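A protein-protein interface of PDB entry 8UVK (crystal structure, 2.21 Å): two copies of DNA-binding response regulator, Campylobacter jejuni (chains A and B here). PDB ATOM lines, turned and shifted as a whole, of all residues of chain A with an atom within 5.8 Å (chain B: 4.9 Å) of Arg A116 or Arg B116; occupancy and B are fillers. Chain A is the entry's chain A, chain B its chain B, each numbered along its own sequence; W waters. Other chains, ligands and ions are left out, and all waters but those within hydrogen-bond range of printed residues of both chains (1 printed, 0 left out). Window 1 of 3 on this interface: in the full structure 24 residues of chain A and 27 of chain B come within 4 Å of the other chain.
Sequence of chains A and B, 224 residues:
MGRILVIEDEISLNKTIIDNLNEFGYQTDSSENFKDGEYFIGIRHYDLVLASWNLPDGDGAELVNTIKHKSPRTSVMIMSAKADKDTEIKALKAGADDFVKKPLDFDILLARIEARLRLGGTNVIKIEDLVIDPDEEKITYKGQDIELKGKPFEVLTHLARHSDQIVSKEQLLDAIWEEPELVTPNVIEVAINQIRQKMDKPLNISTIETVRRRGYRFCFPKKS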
ATOM      1  N   LEU A  48     -20.916  -9.254   6.918  1.00  0.00           N
ATOM      2  CA  LEU A  48     -20.260 -10.517   7.222  1.00  0.00           C
ATOM      3  C   LEU A  48     -21.217 -11.520   7.835  1.00  0.00           C
ATOM      4  O   LEU A  48     -22.181 -11.142   8.498  1.00  0.00           O
ATOM      5  CB  LEU A  48     -19.074 -10.280   8.162  1.00  0.00           C
ATOM      6  CG  LEU A  48     -18.124 -11.444   8.456  1.00  0.00           C
ATOM      7  CD1 LEU A  48     -16.711 -10.939   8.693  1.00  0.00           C
ATOM      8  CD2 LEU A  48     -18.603 -12.286   9.630  1.00  0.00           C
ATOM      9  N   SER A  75     -19.080 -11.366   3.492  1.00  0.00           N
ATOM     10  CA  SER A  75     -17.998 -12.268   3.848  1.00  0.00           C
ATOM     11  C   SER A  75     -18.534 -13.418   4.668  1.00  0.00           C
ATOM     12  O   SER A  75     -19.367 -13.222   5.547  1.00  0.00           O
ATOM     13  CB  SER A  75     -16.922 -11.532   4.641  1.00  0.00           C
ATOM     14  OG  SER A  75     -15.867 -12.409   4.991  1.00  0.00           O
ATOM     15  N   MET A  77     -17.645 -16.368   7.314  1.00  0.00           N
ATOM     16  CA  MET A  77     -16.663 -16.912   8.237  1.00  0.00           C
ATOM     17  C   MET A  77     -17.240 -18.156   8.872  1.00  0.00           C
ATOM     18  O   MET A  77     -18.355 -18.134   9.386  1.00  0.00           O
ATOM     19  CB  MET A  77     -16.292 -15.889   9.303  1.00  0.00           C
ATOM     20  CG  MET A  77     -15.298 -16.396  10.332  1.00  0.00           C
ATOM     21  SD  MET A  77     -14.801 -15.086  11.462  1.00  0.00           S
ATOM     22  CE  MET A  77     -14.033 -13.934  10.330  1.00  0.00           C
ATOM     23  N   ASP A  97     -14.487 -17.246   3.383  1.00  0.00           N
ATOM     24  CA  ASP A  97     -13.428 -16.248   3.360  1.00  0.00           C
ATOM     25  C   ASP A  97     -12.481 -16.442   4.529  1.00  0.00           C
ATOM     26  O   ASP A  97     -11.332 -16.011   4.478  1.00  0.00           O
ATOM     27  CB  ASP A  97     -14.032 -14.848   3.381  1.00  0.00           C
ATOM     28  CG  ASP A  97     -15.005 -14.620   2.244  1.00  0.00           C
ATOM     29  OD1 ASP A  97     -15.109 -15.501   1.365  1.00  0.00           O
ATOM     30  OD2 ASP A  97     -15.663 -13.561   2.224  1.00  0.00           O
ATOM     31  N   ASP A  98     -12.956 -17.090   5.586  1.00  0.00           N
ATOM     32  CA  ASP A  98     -12.089 -17.379   6.719  1.00  0.00           C
ATOM     33  C   ASP A  98     -12.653 -18.520   7.551  1.00  0.00           C
ATOM     34  O   ASP A  98     -13.862 -18.735   7.579  1.00  0.00           O
ATOM     35  CB  ASP A  98     -11.891 -16.130   7.579  1.00  0.00           C
ATOM     36  CG  ASP A  98     -10.672 -16.223   8.475  1.00  0.00           C
ATOM     37  OD1 ASP A  98     -10.003 -17.278   8.471  1.00  0.00           O
ATOM     38  OD2 ASP A  98     -10.377 -15.238   9.180  1.00  0.00           O
ATOM     39  N   ALA A 111     -10.711  -9.426  16.106  1.00  0.00           N
ATOM     40  CA  ALA A 111      -9.627  -8.895  15.283  1.00  0.00           C
ATOM     41  C   ALA A 111      -9.725  -9.364  13.828  1.00  0.00           C
ATOM     42  O   ALA A 111      -9.438  -8.584  12.916  1.00  0.00           O
ATOM     43  CB  ALA A 111      -8.270  -9.281  15.861  1.00  0.00           C
ATOM     44  N   ARG A 112     -10.135 -10.605  13.609  1.00  0.00           N
ATOM     45  CA  ARG A 112     -10.255 -11.116  12.253  1.00  0.00           C
ATOM     46  C   ARG A 112     -11.434 -10.483  11.534  1.00  0.00           C
ATOM     47  O   ARG A 112     -11.325 -10.104  10.372  1.00  0.00           O
ATOM     48  CB  ARG A 112     -10.382 -12.640  12.253  1.00  0.00           C
ATOM     49  CG  ARG A 112      -9.079 -13.355  12.563  1.00  0.00           C
ATOM     50  CD  ARG A 112      -9.149 -14.833  12.225  1.00  0.00           C
ATOM     51  NE  ARG A 112      -7.818 -15.430  12.192  1.00  0.00           N
ATOM     52  CZ  ARG A 112      -7.049 -15.473  11.109  1.00  0.00           C
ATOM     53  NH1 ARG A 112      -7.481 -14.957   9.967  1.00  0.00           N
ATOM     54  NH2 ARG A 112      -5.849 -16.031  11.167  1.00  0.00           N
ATOM     55  N   ILE A 113     -12.559 -10.361  12.224  1.00  0.00           N
ATOM     56  CA  ILE A 113     -13.723  -9.736  11.625  1.00  0.00           C
ATOM     57  C   ILE A 113     -13.362  -8.326  11.222  1.00  0.00           C
ATOM     58  O   ILE A 113     -13.668  -7.889  10.116  1.00  0.00           O
ATOM     59  CB  ILE A 113     -14.908  -9.711  12.598  1.00  0.00           C
ATOM     60  CG1 ILE A 113     -15.339 -11.139  12.930  1.00  0.00           C
ATOM     61  CG2 ILE A 113     -16.066  -8.923  12.009  1.00  0.00           C
ATOM     62  CD1 ILE A 113     -16.498 -11.221  13.896  1.00  0.00           C
ATOM     63  N   GLU A 114     -12.691  -7.616  12.115  1.00  0.00           N
ATOM     64  CA  GLU A 114     -12.256  -6.270  11.800  1.00  0.00           C
ATOM     65  C   GLU A 114     -11.444  -6.281  10.518  1.00  0.00           C
ATOM     66  O   GLU A 114     -11.775  -5.587   9.560  1.00  0.00           O
ATOM     67  CB  GLU A 114     -11.426  -5.706  12.945  1.00  0.00           C
ATOM     68  CG  GLU A 114     -10.961  -4.277  12.737  1.00  0.00           C
ATOM     69  CD  GLU A 114     -10.054  -3.805  13.853  1.00  0.00           C
ATOM     70  OE1 GLU A 114      -9.640  -4.649  14.672  1.00  0.00           O
ATOM     71  OE2 GLU A 114      -9.757  -2.594  13.912  1.00  0.00           O
ATOM     72  N   ALA A 115     -10.379  -7.075  10.496  1.00  0.00           N
ATOM     73  CA  ALA A 115      -9.542  -7.146   9.304  1.00  0.00           C
ATOM     74  C   ALA A 115     -10.353  -7.547   8.078  1.00  0.00           C
ATOM     75  O   ALA A 115     -10.085  -7.075   6.968  1.00  0.00           O
ATOM     76  CB  ALA A 115      -8.382  -8.127   9.535  1.00  0.00           C
ATOM     77  N   ARG A 116     -11.357  -8.396   8.265  1.00  0.00           N
ATOM     78  CA  ARG A 116     -12.127  -8.868   7.131  1.00  0.00           C
ATOM     79  C   ARG A 116     -13.038  -7.770   6.585  1.00  0.00           C
ATOM     80  O   ARG A 116     -13.371  -7.774   5.390  1.00  0.00           O
ATOM     81  CB  ARG A 116     -12.913 -10.105   7.543  1.00  0.00           C
ATOM     82  CG  ARG A 116     -13.338 -10.944   6.385  1.00  0.00           C
ATOM     83  CD  ARG A 116     -12.171 -11.296   5.450  1.00  0.00           C
ATOM     84  NE  ARG A 116     -11.137 -12.106   6.084  1.00  0.00           N
ATOM     85  CZ  ARG A 116      -9.862 -11.754   6.177  1.00  0.00           C
ATOM     86  NH1 ARG A 116      -9.431 -10.592   5.728  1.00  0.00           N
ATOM     87  NH2 ARG A 116      -8.999 -12.587   6.746  1.00  0.00           N
ATOM     88  N   LEU A 117     -13.437  -6.813   7.429  1.00  0.00           N
ATOM     89  CA  LEU A 117     -14.227  -5.665   6.998  1.00  0.00           C
ATOM     90  C   LEU A 117     -13.407  -4.378   6.886  1.00  0.00           C
ATOM     91  O   LEU A 117     -13.986  -3.303   6.757  1.00  0.00           O
ATOM     92  CB  LEU A 117     -15.406  -5.447   7.950  1.00  0.00           C
ATOM     93  CG  LEU A 117     -16.250  -6.702   8.128  1.00  0.00           C
ATOM     94  CD1 LEU A 117     -17.369  -6.494   9.126  1.00  0.00           C
ATOM     95  CD2 LEU A 117     -16.769  -7.149   6.760  1.00  0.00           C
ATOM     96  N   ARG A 118     -12.079  -4.451   6.933  1.00  0.00           N
ATOM     97  CA  ARG A 118     -11.270  -3.256   6.705  1.00  0.00           C
ATOM     98  C   ARG A 118     -11.325  -2.790   5.243  1.00  0.00           C
ATOM     99  O   ARG A 118     -10.992  -3.537   4.311  1.00  0.00           O
ATOM    100  CB  ARG A 118      -9.817  -3.491   7.107  1.00  0.00           C
ATOM    101  CG  ARG A 118      -9.424  -2.650   8.300  1.00  0.00           C
ATOM    102  CD  ARG A 118      -7.924  -2.410   8.335  1.00  0.00           C
ATOM    103  NE  ARG A 118      -7.206  -3.651   8.079  1.00  0.00           N
ATOM    104  CZ  ARG A 118      -6.956  -4.576   8.999  1.00  0.00           C
ATOM    105  NH1 ARG A 118      -7.395  -4.454  10.248  1.00  0.00           N
ATOM    106  NH2 ARG A 118      -6.280  -5.663   8.652  1.00  0.00           N
ATOM    107  N   LEU B  48      -0.431 -10.472  -3.487  1.00  0.00           N
ATOM    108  CA  LEU B  48      -0.300 -10.835  -2.083  1.00  0.00           C
ATOM    109  C   LEU B  48       1.136 -10.875  -1.601  1.00  0.00           C
ATOM    110  O   LEU B  48       2.006 -11.411  -2.278  1.00  0.00           O
ATOM    111  CB  LEU B  48      -0.961 -12.196  -1.831  1.00  0.00           C
ATOM    112  CG  LEU B  48      -0.979 -12.755  -0.406  1.00  0.00           C
ATOM    113  CD1 LEU B  48      -2.199 -13.637  -0.196  1.00  0.00           C
ATOM    114  CD2 LEU B  48       0.298 -13.513  -0.078  1.00  0.00           C
ATOM    115  N   SER B  75      -2.904  -7.890  -0.810  1.00  0.00           N
ATOM    116  CA  SER B  75      -3.236  -8.622   0.402  1.00  0.00           C
ATOM    117  C   SER B  75      -1.962  -8.879   1.186  1.00  0.00           C
ATOM    118  O   SER B  75      -0.900  -9.117   0.594  1.00  0.00           O
ATOM    119  CB  SER B  75      -3.928  -9.937   0.057  1.00  0.00           C
ATOM    120  OG  SER B  75      -4.529 -10.479   1.212  1.00  0.00           O
ATOM    121  N   MET B  77      -0.189 -11.151   4.261  1.00  0.00           N
ATOM    122  CA  MET B  77      -0.299 -12.341   5.098  1.00  0.00           C
ATOM    123  C   MET B  77       0.977 -12.511   5.914  1.00  0.00           C
ATOM    124  O   MET B  77       2.076 -12.590   5.359  1.00  0.00           O
ATOM    125  CB  MET B  77      -0.595 -13.580   4.249  1.00  0.00           C
ATOM    126  CG  MET B  77      -0.720 -14.848   5.078  1.00  0.00           C
ATOM    127  SD  MET B  77      -0.968 -16.311   4.072  1.00  0.00           S
ATOM    128  CE  MET B  77      -2.741 -16.102   3.668  1.00  0.00           C
ATOM    129  N   ASP B  97      -4.153  -8.961   6.460  1.00  0.00           N
ATOM    130  CA  ASP B  97      -5.399  -9.667   6.203  1.00  0.00           C
ATOM    131  C   ASP B  97      -5.393 -11.103   6.734  1.00  0.00           C
ATOM    132  O   ASP B  97      -6.476 -11.700   6.854  1.00  0.00           O
ATOM    133  CB  ASP B  97      -5.753  -9.663   4.691  1.00  0.00           C
ATOM    134  CG  ASP B  97      -5.745  -8.243   4.098  1.00  0.00           C
ATOM    135  OD1 ASP B  97      -4.637  -7.749   3.830  1.00  0.00           O
ATOM    136  OD2 ASP B  97      -6.819  -7.618   3.931  1.00  0.00           O
ATOM    137  N   ASP B  98      -4.228 -11.668   7.062  1.00  0.00           N
ATOM    138  CA  ASP B  98      -4.209 -12.996   7.660  1.00  0.00           C
ATOM    139  C   ASP B  98      -2.900 -13.228   8.412  1.00  0.00           C
ATOM    140  O   ASP B  98      -1.892 -12.551   8.192  1.00  0.00           O
ATOM    141  CB  ASP B  98      -4.460 -14.089   6.602  1.00  0.00           C
ATOM    142  CG  ASP B  98      -5.419 -15.165   7.109  1.00  0.00           C
ATOM    143  OD1 ASP B  98      -5.292 -15.600   8.308  1.00  0.00           O
ATOM    144  OD2 ASP B  98      -6.316 -15.554   6.330  1.00  0.00           O
ATOM    145  N   ARG B 112      -5.548 -21.027   2.118  1.00  0.00           N
ATOM    146  CA  ARG B 112      -5.855 -19.698   2.643  1.00  0.00           C
ATOM    147  C   ARG B 112      -5.437 -18.603   1.681  1.00  0.00           C
ATOM    148  O   ARG B 112      -6.168 -17.628   1.501  1.00  0.00           O
ATOM    149  CB  ARG B 112      -5.169 -19.459   3.991  1.00  0.00           C
ATOM    150  CG  ARG B 112      -5.898 -20.045   5.164  1.00  0.00           C
ATOM    151  CD  ARG B 112      -5.335 -19.547   6.492  1.00  0.00           C
ATOM    152  NE  ARG B 112      -6.181 -19.989   7.586  1.00  0.00           N
ATOM    153  CZ  ARG B 112      -7.311 -19.388   7.941  1.00  0.00           C
ATOM    154  NH1 ARG B 112      -7.743 -18.288   7.323  1.00  0.00           N
ATOM    155  NH2 ARG B 112      -8.033 -19.910   8.926  1.00  0.00           N
ATOM    156  N   ILE B 113      -4.236 -18.720   1.119  1.00  0.00           N
ATOM    157  CA  ILE B 113      -3.834 -17.850   0.018  1.00  0.00           C
ATOM    158  C   ILE B 113      -4.901 -17.837  -1.066  1.00  0.00           C
ATOM    159  O   ILE B 113      -5.371 -16.777  -1.493  1.00  0.00           O
ATOM    160  CB  ILE B 113      -2.479 -18.287  -0.546  1.00  0.00           C
ATOM    161  CG1 ILE B 113      -1.412 -18.028   0.492  1.00  0.00           C
ATOM    162  CG2 ILE B 113      -2.187 -17.492  -1.787  1.00  0.00           C
ATOM    163  CD1 ILE B 113      -0.035 -18.372   0.052  1.00  0.00           C
ATOM    164  N   GLU B 114      -5.345 -19.013  -1.482  1.00  0.00           N
ATOM    165  CA  GLU B 114      -6.354 -19.075  -2.532  1.00  0.00           C
ATOM    166  C   GLU B 114      -7.648 -18.399  -2.106  1.00  0.00           C
ATOM    167  O   GLU B 114      -8.328 -17.783  -2.929  1.00  0.00           O
ATOM    168  CB  GLU B 114      -6.607 -20.526  -2.897  1.00  0.00           C
ATOM    169  CG  GLU B 114      -7.421 -20.809  -4.075  1.00  0.00           C
ATOM    170  CD  GLU B 114      -8.261 -22.033  -3.854  1.00  0.00           C
ATOM    171  OE1 GLU B 114      -7.720 -22.951  -3.207  1.00  0.00           O
ATOM    172  OE2 GLU B 114      -9.391 -22.157  -4.395  1.00  0.00           O
ATOM    173  N   ALA B 115      -8.028 -18.524  -0.833  1.00  0.00           N
ATOM    174  CA  ALA B 115      -9.228 -17.843  -0.355  1.00  0.00           C
ATOM    175  C   ALA B 115      -9.043 -16.323  -0.343  1.00  0.00           C
ATOM    176  O   ALA B 115     -10.002 -15.583  -0.573  1.00  0.00           O
ATOM    177  CB  ALA B 115      -9.611 -18.331   1.054  1.00  0.00           C
ATOM    178  N   ARG B 116      -7.841 -15.827  -0.038  1.00  0.00           N
ATOM    179  CA  ARG B 116      -7.685 -14.380  -0.092  1.00  0.00           C
ATOM    180  C   ARG B 116      -7.737 -13.894  -1.537  1.00  0.00           C
ATOM    181  O   ARG B 116      -8.357 -12.863  -1.822  1.00  0.00           O
ATOM    182  CB  ARG B 116      -6.382 -13.910   0.566  1.00  0.00           C
ATOM    183  CG  ARG B 116      -6.128 -14.363   1.978  1.00  0.00           C
ATOM    184  CD  ARG B 116      -6.594 -13.326   3.045  1.00  0.00           C
ATOM    185  NE  ARG B 116      -8.039 -13.153   3.018  1.00  0.00           N
ATOM    186  CZ  ARG B 116      -8.896 -13.973   3.599  1.00  0.00           C
ATOM    187  NH1 ARG B 116      -8.484 -14.949   4.393  1.00  0.00           N
ATOM    188  NH2 ARG B 116     -10.195 -13.813   3.377  1.00  0.00           N
ATOM    189  N   LEU B 117      -7.121 -14.629  -2.471  1.00  0.00           N
ATOM    190  CA  LEU B 117      -7.051 -14.128  -3.848  1.00  0.00           C
ATOM    191  C   LEU B 117      -8.366 -14.272  -4.604  1.00  0.00           C
ATOM    192  O   LEU B 117      -8.492 -13.712  -5.685  1.00  0.00           O
ATOM    193  CB  LEU B 117      -5.897 -14.786  -4.618  1.00  0.00           C
ATOM    194  CG  LEU B 117      -4.515 -14.509  -3.966  1.00  0.00           C
ATOM    195  CD1 LEU B 117      -3.358 -15.096  -4.756  1.00  0.00           C
ATOM    196  CD2 LEU B 117      -4.243 -13.043  -3.663  1.00  0.00           C
ATOM    197  N   ARG B 118      -9.379 -14.926  -4.042  1.00  0.00           N
ATOM    198  CA  ARG B 118     -10.700 -14.938  -4.659  1.00  0.00           C
ATOM    199  C   ARG B 118     -11.434 -13.597  -4.529  1.00  0.00           C
ATOM    200  O   ARG B 118     -12.522 -13.455  -5.106  1.00  0.00           O
ATOM    201  CB  ARG B 118     -11.562 -16.038  -4.028  1.00  0.00           C
ATOM    202  CG  ARG B 118     -11.111 -17.484  -4.326  1.00  0.00           C
ATOM    203  CD  ARG B 118     -12.221 -18.480  -3.980  1.00  0.00           C
ATOM    204  NE  ARG B 118     -12.534 -18.460  -2.558  1.00  0.00           N
ATOM    205  CZ  ARG B 118     -12.318 -19.462  -1.701  1.00  0.00           C
ATOM    206  NH1 ARG B 118     -11.814 -20.627  -2.100  1.00  0.00           N
ATOM    207  NH2 ARG B 118     -12.648 -19.301  -0.415  1.00  0.00           N
ATOM    208  N   LEU B 119     -10.887 -12.642  -3.765  1.00  0.00           N
ATOM    209  CA  LEU B 119     -11.481 -11.311  -3.583  1.00  0.00           C
ATOM    210  C   LEU B 119     -12.970 -11.401  -3.241  1.00  0.00           C
ATOM    211  O   LEU B 119     -13.802 -10.655  -3.770  1.00  0.00           O
ATOM    212  CB  LEU B 119     -11.245 -10.438  -4.828  1.00  0.00           C
ATOM    213  CG  LEU B 119      -9.771 -10.093  -5.121  1.00  0.00           C
ATOM    214  CD1 LEU B 119      -9.590  -8.762  -5.918  1.00  0.00           C
ATOM    215  CD2 LEU B 119      -8.963 -10.009  -3.843  1.00  0.00           C
HETATM  216  O   HOH W   1      -7.713  -6.382   6.630  1.00  0.00           O
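Water W1 lies within hydrogen-bond range of the backbone carbonyl oxygen (O) of Ala A115 (2.5 Å), the guanidinium group (NH2) of Arg A118 (2.6 Å) and the side-chain carboxylate (OD2) of Asp B97 (3.1 Å).
Asp A97 touches Arg B116, and with the chains exchanged Arg A116 touches Asp B97.
Asp A98 touches Arg B112, and with the chains exchanged Arg A112 touches Asp B98.
Arg B116 touches its own counterpart, Arg A116.
OG of Ser A75 lies within hydrogen-bond range of OD2 of Asp A97, 3.0 Å away.
The side-chain carboxylate of Asp A98 is in salt-bridge range of the guanidinium group of Arg A116.
The side-chain carboxylate (OD2) of Asp B98 is in salt-bridge range of the guanidinium group (NH1) of Arg B112, 3.2 Å away.
The side-chain carboxylate (OD2) of Asp B98 is in salt-bridge range of the guanidinium group (NH1) of Arg B116.
NH1 of Arg A112 lies within salt-bridge range of OD2 of Asp A98 (3.0 Å).
Arg A116 touches just these residues of chain B: Asp B97 (2.7 Å) and Arg B116 (3.3 Å).
Of chain A, only Asp A97 (2.7 Å) and Arg A116 (3.3 Å) come within 4 Å of Arg B116.
Printed residues of chain A within 4 Å of Asp B97: Arg A116 (2.7 Å).
Printed residues of chain B within 4 Å of Asp A97: Arg B116 (2.7 Å).
Printed residues of chain A within 4 Å of Arg B112: Asp A98.
Arg B118 touches none of the printed residues of chain A.
Ser A75 touches none of the printed residues of chain B.
The nearest residue of chain B that does not touch Arg A116 is Asp B98 (4.02 Å).
The nearest residue of chain A that does not touch Arg B116 is Asp A98 (4.8 Å).
The nearest printed residue of chain A that does not touch Arg B112 is Arg A112 (4.3 Å).
The backbone carbonyl oxygen (O) of Asp A97 lies within hydrogen-bond range of the guanidinium group (NH2) of Arg B116, 2.7 Å away.
NH2 of Arg B116 sits close to NE of Arg A116 (3.3 Å).
The guanidinium group (NH1) of Arg B112 lies within salt-bridge range of the side-chain carboxylate (OD1) of Asp A98, 2.7 Å away.
The backbone carbonyl oxygen (O) of Asp B97 is in hydrogen-bond range of the guanidinium group (NH2) of Arg A116 (2.7 Å).
NH1 of Arg A112 lies within salt-bridge range of OD1 of Asp B98, 2.8 Å away.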
